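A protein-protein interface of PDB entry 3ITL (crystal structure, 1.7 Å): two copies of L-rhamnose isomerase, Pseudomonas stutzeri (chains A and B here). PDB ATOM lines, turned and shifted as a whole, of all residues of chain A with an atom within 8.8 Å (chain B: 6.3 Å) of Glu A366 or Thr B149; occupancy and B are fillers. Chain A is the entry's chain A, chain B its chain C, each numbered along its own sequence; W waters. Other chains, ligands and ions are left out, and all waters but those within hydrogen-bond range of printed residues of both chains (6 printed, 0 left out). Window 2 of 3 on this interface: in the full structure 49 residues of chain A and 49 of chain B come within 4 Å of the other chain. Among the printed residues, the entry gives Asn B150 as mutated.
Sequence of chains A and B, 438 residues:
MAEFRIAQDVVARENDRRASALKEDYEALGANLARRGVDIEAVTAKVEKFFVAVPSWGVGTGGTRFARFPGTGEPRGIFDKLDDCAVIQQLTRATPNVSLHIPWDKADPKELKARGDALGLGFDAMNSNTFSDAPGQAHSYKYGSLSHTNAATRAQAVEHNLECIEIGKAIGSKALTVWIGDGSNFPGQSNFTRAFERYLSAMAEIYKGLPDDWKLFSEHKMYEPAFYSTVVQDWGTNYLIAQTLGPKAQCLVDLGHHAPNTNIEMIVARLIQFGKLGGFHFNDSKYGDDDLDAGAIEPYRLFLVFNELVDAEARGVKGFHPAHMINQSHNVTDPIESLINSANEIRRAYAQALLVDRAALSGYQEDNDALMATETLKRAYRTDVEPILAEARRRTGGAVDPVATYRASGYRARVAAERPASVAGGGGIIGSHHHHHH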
ATOM      1  N   ALA A 359      10.760 -14.884  16.678  1.00  0.00           N
ATOM      2  CA  ALA A 359      10.494 -15.852  15.622  1.00  0.00           C
ATOM      3  C   ALA A 359      10.165 -15.014  14.386  1.00  0.00           C
ATOM      4  O   ALA A 359      10.691 -15.244  13.297  1.00  0.00           O
ATOM      5  CB  ALA A 359       9.309 -16.738  16.000  1.00  0.00           C
ATOM      6  N   ALA A 360       9.297 -14.025  14.569  1.00  0.00           N
ATOM      7  CA  ALA A 360       8.910 -13.139  13.484  1.00  0.00           C
ATOM      8  C   ALA A 360      10.113 -12.316  13.042  1.00  0.00           C
ATOM      9  O   ALA A 360      10.360 -12.152  11.848  1.00  0.00           O
ATOM     10  CB  ALA A 360       7.790 -12.215  13.934  1.00  0.00           C
ATOM     11  N   LEU A 361      10.868 -11.803  14.008  1.00  0.00           N
ATOM     12  CA  LEU A 361      12.031 -10.986  13.680  1.00  0.00           C
ATOM     13  C   LEU A 361      13.039 -11.740  12.815  1.00  0.00           C
ATOM     14  O   LEU A 361      13.553 -11.195  11.838  1.00  0.00           O
ATOM     15  CB  LEU A 361      12.717 -10.487  14.958  1.00  0.00           C
ATOM     16  CG  LEU A 361      13.924  -9.563  14.751  1.00  0.00           C
ATOM     17  CD1 LEU A 361      13.506  -8.344  13.942  1.00  0.00           C
ATOM     18  CD2 LEU A 361      14.489  -9.142  16.102  1.00  0.00           C
ATOM     19  N   SER A 362      13.316 -12.993  13.165  1.00  0.00           N
ATOM     20  CA  SER A 362      14.270 -13.786  12.396  1.00  0.00           C
ATOM     21  C   SER A 362      13.815 -13.942  10.946  1.00  0.00           C
ATOM     22  O   SER A 362      14.631 -13.900  10.027  1.00  0.00           O
ATOM     23  CB  SER A 362      14.469 -15.161  13.041  1.00  0.00           C
ATOM     24  OG  SER A 362      13.237 -15.842  13.192  1.00  0.00           O
ATOM     25  N   GLY A 363      12.513 -14.111  10.743  1.00  0.00           N
ATOM     26  CA  GLY A 363      11.993 -14.253   9.395  1.00  0.00           C
ATOM     27  C   GLY A 363      12.153 -12.968   8.601  1.00  0.00           C
ATOM     28  O   GLY A 363      12.561 -12.988   7.438  1.00  0.00           O
ATOM     29  N   TYR A 364      11.835 -11.840   9.228  1.00  0.00           N
ATOM     30  CA  TYR A 364      11.953 -10.557   8.551  1.00  0.00           C
ATOM     31  C   TYR A 364      13.410 -10.206   8.251  1.00  0.00           C
ATOM     32  O   TYR A 364      13.695  -9.522   7.270  1.00  0.00           O
ATOM     33  CB  TYR A 364      11.298  -9.447   9.383  1.00  0.00           C
ATOM     34  CG  TYR A 364       9.797  -9.592   9.518  1.00  0.00           C
ATOM     35  CD1 TYR A 364       8.997  -9.833   8.399  1.00  0.00           C
ATOM     36  CD2 TYR A 364       9.172  -9.472  10.761  1.00  0.00           C
ATOM     37  CE1 TYR A 364       7.615  -9.950   8.511  1.00  0.00           C
ATOM     38  CE2 TYR A 364       7.786  -9.586  10.885  1.00  0.00           C
ATOM     39  CZ  TYR A 364       7.016  -9.826   9.756  1.00  0.00           C
ATOM     40  OH  TYR A 364       5.649  -9.931   9.866  1.00  0.00           O
ATOM     41  N   GLN A 365      14.331 -10.669   9.092  1.00  0.00           N
ATOM     42  CA  GLN A 365      15.746 -10.394   8.866  1.00  0.00           C
ATOM     43  C   GLN A 365      16.245 -11.230   7.690  1.00  0.00           C
ATOM     44  O   GLN A 365      16.964 -10.732   6.826  1.00  0.00           O
ATOM     45  CB  GLN A 365      16.569 -10.703  10.123  1.00  0.00           C
ATOM     46  CG  GLN A 365      16.240  -9.785  11.299  1.00  0.00           C
ATOM     47  CD  GLN A 365      17.008 -10.124  12.565  1.00  0.00           C
ATOM     48  OE1 GLN A 365      17.244 -11.293  12.870  1.00  0.00           O
ATOM     49  NE2 GLN A 365      17.379  -9.100  13.324  1.00  0.00           N
ATOM     50  N   GLU A 366      15.852 -12.499   7.654  1.00  0.00           N
ATOM     51  CA  GLU A 366      16.268 -13.392   6.574  1.00  0.00           C
ATOM     52  C   GLU A 366      15.742 -12.933   5.213  1.00  0.00           C
ATOM     53  O   GLU A 366      16.437 -13.047   4.202  1.00  0.00           O
ATOM     54  CB  GLU A 366      15.782 -14.820   6.856  1.00  0.00           C
ATOM     55  CG  GLU A 366      16.126 -15.832   5.766  1.00  0.00           C
ATOM     56  CD  GLU A 366      17.618 -16.120   5.655  1.00  0.00           C
ATOM     57  OE1 GLU A 366      18.007 -16.856   4.723  1.00  0.00           O
ATOM     58  OE2 GLU A 366      18.401 -15.620   6.494  1.00  0.00           O
ATOM     59  N   ASP A 367      14.520 -12.407   5.196  1.00  0.00           N
ATOM     60  CA  ASP A 367      13.881 -11.942   3.966  1.00  0.00           C
ATOM     61  C   ASP A 367      14.166 -10.480   3.632  1.00  0.00           C
ATOM     62  O   ASP A 367      13.616  -9.940   2.672  1.00  0.00           O
ATOM     63  CB  ASP A 367      12.369 -12.142   4.071  1.00  0.00           C
ATOM     64  CG  ASP A 367      11.970 -13.605   4.058  1.00  0.00           C
ATOM     65  OD1 ASP A 367      10.832 -13.908   4.471  1.00  0.00           O
ATOM     66  OD2 ASP A 367      12.786 -14.449   3.626  1.00  0.00           O
ATOM     67  N   ASN A 368      15.026  -9.850   4.426  1.00  0.00           N
ATOM     68  CA  ASN A 368      15.383  -8.449   4.240  1.00  0.00           C
ATOM     69  C   ASN A 368      14.161  -7.532   4.185  1.00  0.00           C
ATOM     70  O   ASN A 368      14.088  -6.620   3.359  1.00  0.00           O
ATOM     71  CB  ASN A 368      16.230  -8.273   2.977  1.00  0.00           C
ATOM     72  CG  ASN A 368      17.583  -8.951   3.090  1.00  0.00           C
ATOM     73  OD1 ASN A 368      17.862  -9.930   2.395  1.00  0.00           O
ATOM     74  ND2 ASN A 368      18.426  -8.439   3.976  1.00  0.00           N
ATOM     75  N   ASP A 369      13.201  -7.793   5.066  1.00  0.00           N
ATOM     76  CA  ASP A 369      11.986  -6.986   5.168  1.00  0.00           C
ATOM     77  C   ASP A 369      12.303  -5.996   6.294  1.00  0.00           C
ATOM     78  O   ASP A 369      11.862  -6.174   7.430  1.00  0.00           O
ATOM     79  CB  ASP A 369      10.799  -7.873   5.565  1.00  0.00           C
ATOM     80  CG  ASP A 369       9.463  -7.149   5.478  1.00  0.00           C
ATOM     81  OD1 ASP A 369       9.451  -5.902   5.445  1.00  0.00           O
ATOM     82  OD2 ASP A 369       8.416  -7.835   5.459  1.00  0.00           O
ATOM     83  N   ALA A 370      13.085  -4.970   5.970  1.00  0.00           N
ATOM     84  CA  ALA A 370      13.510  -3.971   6.948  1.00  0.00           C
ATOM     85  C   ALA A 370      12.372  -3.272   7.675  1.00  0.00           C
ATOM     86  O   ALA A 370      12.456  -3.031   8.885  1.00  0.00           O
ATOM     87  CB  ALA A 370      14.408  -2.932   6.272  1.00  0.00           C
ATOM     88  N   ALA A 373      10.808  -5.667  10.126  1.00  0.00           N
ATOM     89  CA  ALA A 373      11.785  -6.027  11.145  1.00  0.00           C
ATOM     90  C   ALA A 373      11.805  -4.941  12.219  1.00  0.00           C
ATOM     91  O   ALA A 373      11.734  -5.233  13.417  1.00  0.00           O
ATOM     92  CB  ALA A 373      13.166  -6.176  10.524  1.00  0.00           C
ATOM     93  N   TYR B 143      20.614  -5.086  -0.358  1.00  0.00           N
ATOM     94  CA  TYR B 143      20.598  -5.438   1.060  1.00  0.00           C
ATOM     95  C   TYR B 143      21.921  -6.006   1.555  1.00  0.00           C
ATOM     96  O   TYR B 143      21.972  -6.679   2.584  1.00  0.00           O
ATOM     97  CB  TYR B 143      19.476  -6.440   1.328  1.00  0.00           C
ATOM     98  CG  TYR B 143      18.106  -5.909   0.980  1.00  0.00           C
ATOM     99  CD1 TYR B 143      17.565  -4.823   1.665  1.00  0.00           C
ATOM    100  CD2 TYR B 143      17.350  -6.490  -0.038  1.00  0.00           C
ATOM    101  CE1 TYR B 143      16.306  -4.328   1.346  1.00  0.00           C
ATOM    102  CE2 TYR B 143      16.088  -6.000  -0.368  1.00  0.00           C
ATOM    103  CZ  TYR B 143      15.573  -4.919   0.331  1.00  0.00           C
ATOM    104  OH  TYR B 143      14.326  -4.428   0.015  1.00  0.00           O
ATOM    105  N   SER B 145      26.235  -7.407   0.440  1.00  0.00           N
ATOM    106  CA  SER B 145      27.049  -8.143  -0.516  1.00  0.00           C
ATOM    107  C   SER B 145      27.746  -9.308   0.182  1.00  0.00           C
ATOM    108  O   SER B 145      27.198 -10.413   0.263  1.00  0.00           O
ATOM    109  CB  SER B 145      28.076  -7.197  -1.155  1.00  0.00           C
ATOM    110  OG  SER B 145      28.798  -6.473  -0.172  1.00  0.00           O
ATOM    111  N   SER B 147      28.066  -9.774   3.194  1.00  0.00           N
ATOM    112  CA  SER B 147      27.329 -10.159   4.397  1.00  0.00           C
ATOM    113  C   SER B 147      25.829 -10.330   4.144  1.00  0.00           C
ATOM    114  O   SER B 147      25.042 -10.447   5.085  1.00  0.00           O
ATOM    115  CB  SER B 147      27.546  -9.133   5.520  1.00  0.00           C
ATOM    116  OG  SER B 147      26.918  -7.898   5.229  1.00  0.00           O
ATOM    117  N   HIS B 148      25.441 -10.348   2.870  1.00  0.00           N
ATOM    118  CA  HIS B 148      24.043 -10.513   2.479  1.00  0.00           C
ATOM    119  C   HIS B 148      23.504 -11.838   3.041  1.00  0.00           C
ATOM    120  O   HIS B 148      24.250 -12.811   3.172  1.00  0.00           O
ATOM    121  CB  HIS B 148      23.947 -10.495   0.947  1.00  0.00           C
ATOM    122  CG  HIS B 148      22.561 -10.276   0.420  1.00  0.00           C
ATOM    123  ND1 HIS B 148      21.557 -11.213   0.545  1.00  0.00           N
ATOM    124  CD2 HIS B 148      22.018  -9.232  -0.250  1.00  0.00           C
ATOM    125  CE1 HIS B 148      20.457 -10.755  -0.026  1.00  0.00           C
ATOM    126  NE2 HIS B 148      20.710  -9.556  -0.517  1.00  0.00           N
ATOM    127  N   THR B 149      22.218 -11.875   3.378  1.00  0.00           N
ATOM    128  CA  THR B 149      21.612 -13.088   3.928  1.00  0.00           C
ATOM    129  C   THR B 149      21.521 -14.215   2.905  1.00  0.00           C
ATOM    130  O   THR B 149      21.454 -15.390   3.273  1.00  0.00           O
ATOM    131  CB  THR B 149      20.190 -12.826   4.457  1.00  0.00           C
ATOM    132  OG1 THR B 149      19.376 -12.302   3.402  1.00  0.00           O
ATOM    133  CG2 THR B 149      20.222 -11.839   5.615  1.00  0.00           C
ATOM    134  N   ASN B 150      21.517 -13.849   1.625  1.00  0.00           N
ATOM    135  CA  ASN B 150      21.417 -14.817   0.529  1.00  0.00           C
ATOM    136  C   ASN B 150      22.789 -15.381   0.148  1.00  0.00           C
ATOM    137  O   ASN B 150      23.670 -14.648  -0.295  1.00  0.00           O
ATOM    138  CB  ASN B 150      20.769 -14.142  -0.685  1.00  0.00           C
ATOM    139  CG  ASN B 150      20.508 -15.110  -1.824  1.00  0.00           C
ATOM    140  OD1 ASN B 150      19.756 -16.071  -1.675  1.00  0.00           O
ATOM    141  ND2 ASN B 150      21.130 -14.858  -2.971  1.00  0.00           N
ATOM    142  N   ALA B 151      22.956 -16.692   0.317  1.00  0.00           N
ATOM    143  CA  ALA B 151      24.219 -17.361   0.009  1.00  0.00           C
ATOM    144  C   ALA B 151      24.742 -17.070  -1.399  1.00  0.00           C
ATOM    145  O   ALA B 151      25.929 -16.801  -1.581  1.00  0.00           O
ATOM    146  CB  ALA B 151      24.067 -18.870   0.204  1.00  0.00           C
ATOM    147  N   THR B 153      24.214 -14.507  -3.244  1.00  0.00           N
ATOM    148  CA  THR B 153      24.650 -13.121  -3.348  1.00  0.00           C
ATOM    149  C   THR B 153      26.049 -12.961  -2.761  1.00  0.00           C
ATOM    150  O   THR B 153      26.875 -12.219  -3.297  1.00  0.00           O
ATOM    151  CB  THR B 153      23.664 -12.183  -2.629  1.00  0.00           C
ATOM    152  OG1 THR B 153      22.358 -12.359  -3.190  1.00  0.00           O
ATOM    153  CG2 THR B 153      24.085 -10.723  -2.804  1.00  0.00           C
ATOM    154  N   ARG B 154      26.323 -13.659  -1.662  1.00  0.00           N
ATOM    155  CA  ARG B 154      27.644 -13.581  -1.047  1.00  0.00           C
ATOM    156  C   ARG B 154      28.664 -14.243  -1.978  1.00  0.00           C
ATOM    157  O   ARG B 154      29.780 -13.752  -2.144  1.00  0.00           O
ATOM    158  CB  ARG B 154      27.656 -14.280   0.318  1.00  0.00           C
ATOM    159  CG  ARG B 154      26.726 -13.660   1.359  1.00  0.00           C
ATOM    160  CD  ARG B 154      27.090 -14.127   2.767  1.00  0.00           C
ATOM    161  NE  ARG B 154      26.975 -15.575   2.941  1.00  0.00           N
ATOM    162  CZ  ARG B 154      25.824 -16.227   3.087  1.00  0.00           C
ATOM    163  NH1 ARG B 154      25.820 -17.546   3.239  1.00  0.00           N
ATOM    164  NH2 ARG B 154      24.677 -15.564   3.087  1.00  0.00           N
ATOM    165  N   GLN B 189      16.527  -4.509  11.447  1.00  0.00           N
ATOM    166  CA  GLN B 189      16.668  -4.947  10.058  1.00  0.00           C
ATOM    167  C   GLN B 189      17.735  -6.022   9.925  1.00  0.00           C
ATOM    168  O   GLN B 189      17.553  -7.008   9.206  1.00  0.00           O
ATOM    169  CB  GLN B 189      17.034  -3.767   9.154  1.00  0.00           C
ATOM    170  CG  GLN B 189      17.415  -4.179   7.735  1.00  0.00           C
ATOM    171  CD  GLN B 189      17.846  -3.007   6.875  1.00  0.00           C
ATOM    172  OE1 GLN B 189      18.298  -3.187   5.739  1.00  0.00           O
ATOM    173  NE2 GLN B 189      17.709  -1.802   7.405  1.00  0.00           N
ATOM    174  N   ARG B 198      28.675 -13.718   8.713  1.00  0.00           N
ATOM    175  CA  ARG B 198      28.584 -13.957   7.277  1.00  0.00           C
ATOM    176  C   ARG B 198      29.720 -13.242   6.548  1.00  0.00           C
ATOM    177  O   ARG B 198      30.337 -13.800   5.641  1.00  0.00           O
ATOM    178  CB  ARG B 198      27.228 -13.483   6.734  1.00  0.00           C
ATOM    179  CG  ARG B 198      26.040 -14.292   7.240  1.00  0.00           C
ATOM    180  CD  ARG B 198      24.791 -14.021   6.414  1.00  0.00           C
ATOM    181  NE  ARG B 198      24.231 -12.690   6.636  1.00  0.00           N
ATOM    182  CZ  ARG B 198      23.427 -12.368   7.644  1.00  0.00           C
ATOM    183  NH1 ARG B 198      22.972 -11.126   7.754  1.00  0.00           N
ATOM    184  NH2 ARG B 198      23.068 -13.281   8.541  1.00  0.00           N
HETATM  185  O   HOH W   1      12.968  -3.992   3.031  1.00  0.00           O
HETATM  186  O   HOH W   2      21.048  -9.075   3.626  1.00  0.00           O
HETATM  187  O   HOH W   3      21.493 -15.919   5.973  1.00  0.00           O
HETATM  188  O   HOH W   4      18.733  -9.040   7.875  1.00  0.00           O
HETATM  189  O   HOH W   5      19.083  -5.958   5.021  1.00  0.00           O
HETATM  190  O   HOH W   6      15.486  -6.943   7.378  1.00  0.00           O
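No position is printed for both chains. Of the 8 pairs that touch across the chains among the printed residues, none has its exchanged pair printed and touching as well.
Hydrophobic or aromatic side chains of chain B that line the printed part of chain A: Tyr B143 and His B148. Of the 13 printed residues of chain A, 5 touch a printed residue of chain B. Printed residues of chain A that touch a printed residue of chain B: Gln A365, Glu A366, Asn A368, Ala A370 and Ala A373. Among the printed residues, 8 pairs touch across the chains. Among the printed residues, no Asp or Glu carboxylate lies within 4 Å of a Lys or Arg side-chain nitrogen of the other chain.
ND1 of His B148 lies within hydrogen-bond range of N of Asn B150 (2.8 Å). The backbone carbonyl oxygen (O) of His B148 lies within hydrogen-bond range of the guanidinium group (NH2) of Arg B154, 2.8 Å away. The backbone carbonyl oxygen (O) of His B148 sits at hydrogen-bond distance from the guanidinium group (NE) of Arg B198 (3.5 Å). The backbone carbonyl oxygen (O) of Thr B149 is in hydrogen-bond range of the guanidinium group (NH2) of Arg B154.
Gln A365 touches Thr B149 (O to CG2, 3.6 Å). CG of Gln A365 touches O of Gln B189 (3.7 Å). ND2 of Asn A368 touches CB of Tyr B143, at 3.5 Å. His B148 touches Asn A368. Ala A370 touches Gln B189 (CB to CD, 3.5 Å). Ala A373 touches Gln B189.
Water W4 bridges O of Gln A365 and O of Gln B189. Water W2 lies within hydrogen-bond range of ND2 of Asn A368 (2.7 Å), O of Tyr B143 (2.8 Å) and N of Thr B149 (3.0 Å). Water W3 bridges O of Thr B149 (2.8 Å) and OE2 of Glu A366 (3.1 Å). Water W6 lies within hydrogen-bond range of the backbone carbonyl oxygen of Gln B189 (2.8 Å), the backbone carbonyl oxygen of Tyr A364 (3.1 Å), the backbone NH of Asp A369 (3.4 Å) and the backbone NH of Ala A370 (3.4 Å). Water W5 lies within hydrogen-bond range of ND2 of Asn A368 (2.8 Å) and OE1 of Gln B189 (3.0 Å). Water W1 lies within hydrogen-bond range of the backbone carbonyl oxygen (O) of Asn A368, the backbone NH (N) of Ala A370 and the side-chain hydroxyl (OH) of Tyr B143.
OG1 of Thr B149 is in hydrogen-bond range of O of Glu A366 (3.1 Å). OD1 of Asn A368 sits at hydrogen-bond distance from OG1 of Thr B149 (3.0 Å).
Of the printed residues of chain B, Gln A365 touches Thr B149 (3.6 Å) and Gln B189 (3.7 Å). Glu A366 touches just one residue of chain B: Thr B149. Asp A369 touches none of the printed residues of chain B. Printed residues of chain A within 4 Å of His B148: Asn A368 (3.6 Å). Thr B149 touches three residues of chain A. Ala B151 touches none of the printed residues of chain A. Of the printed residues of chain A, Gln B189 touches Gln A365 (3.7 Å), Ala A370 (3.5 Å) and Ala A373 (3.7 Å). The nearest residue of chain B that does not touch Glu A366 is Asn B150 (5.6 Å). The nearest residue of chain A that does not touch Thr B149 is Asp A367 (5.2 Å). The nearest printed residue of chain B that does not touch Gln A365 is Arg B198 (6.1 Å).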
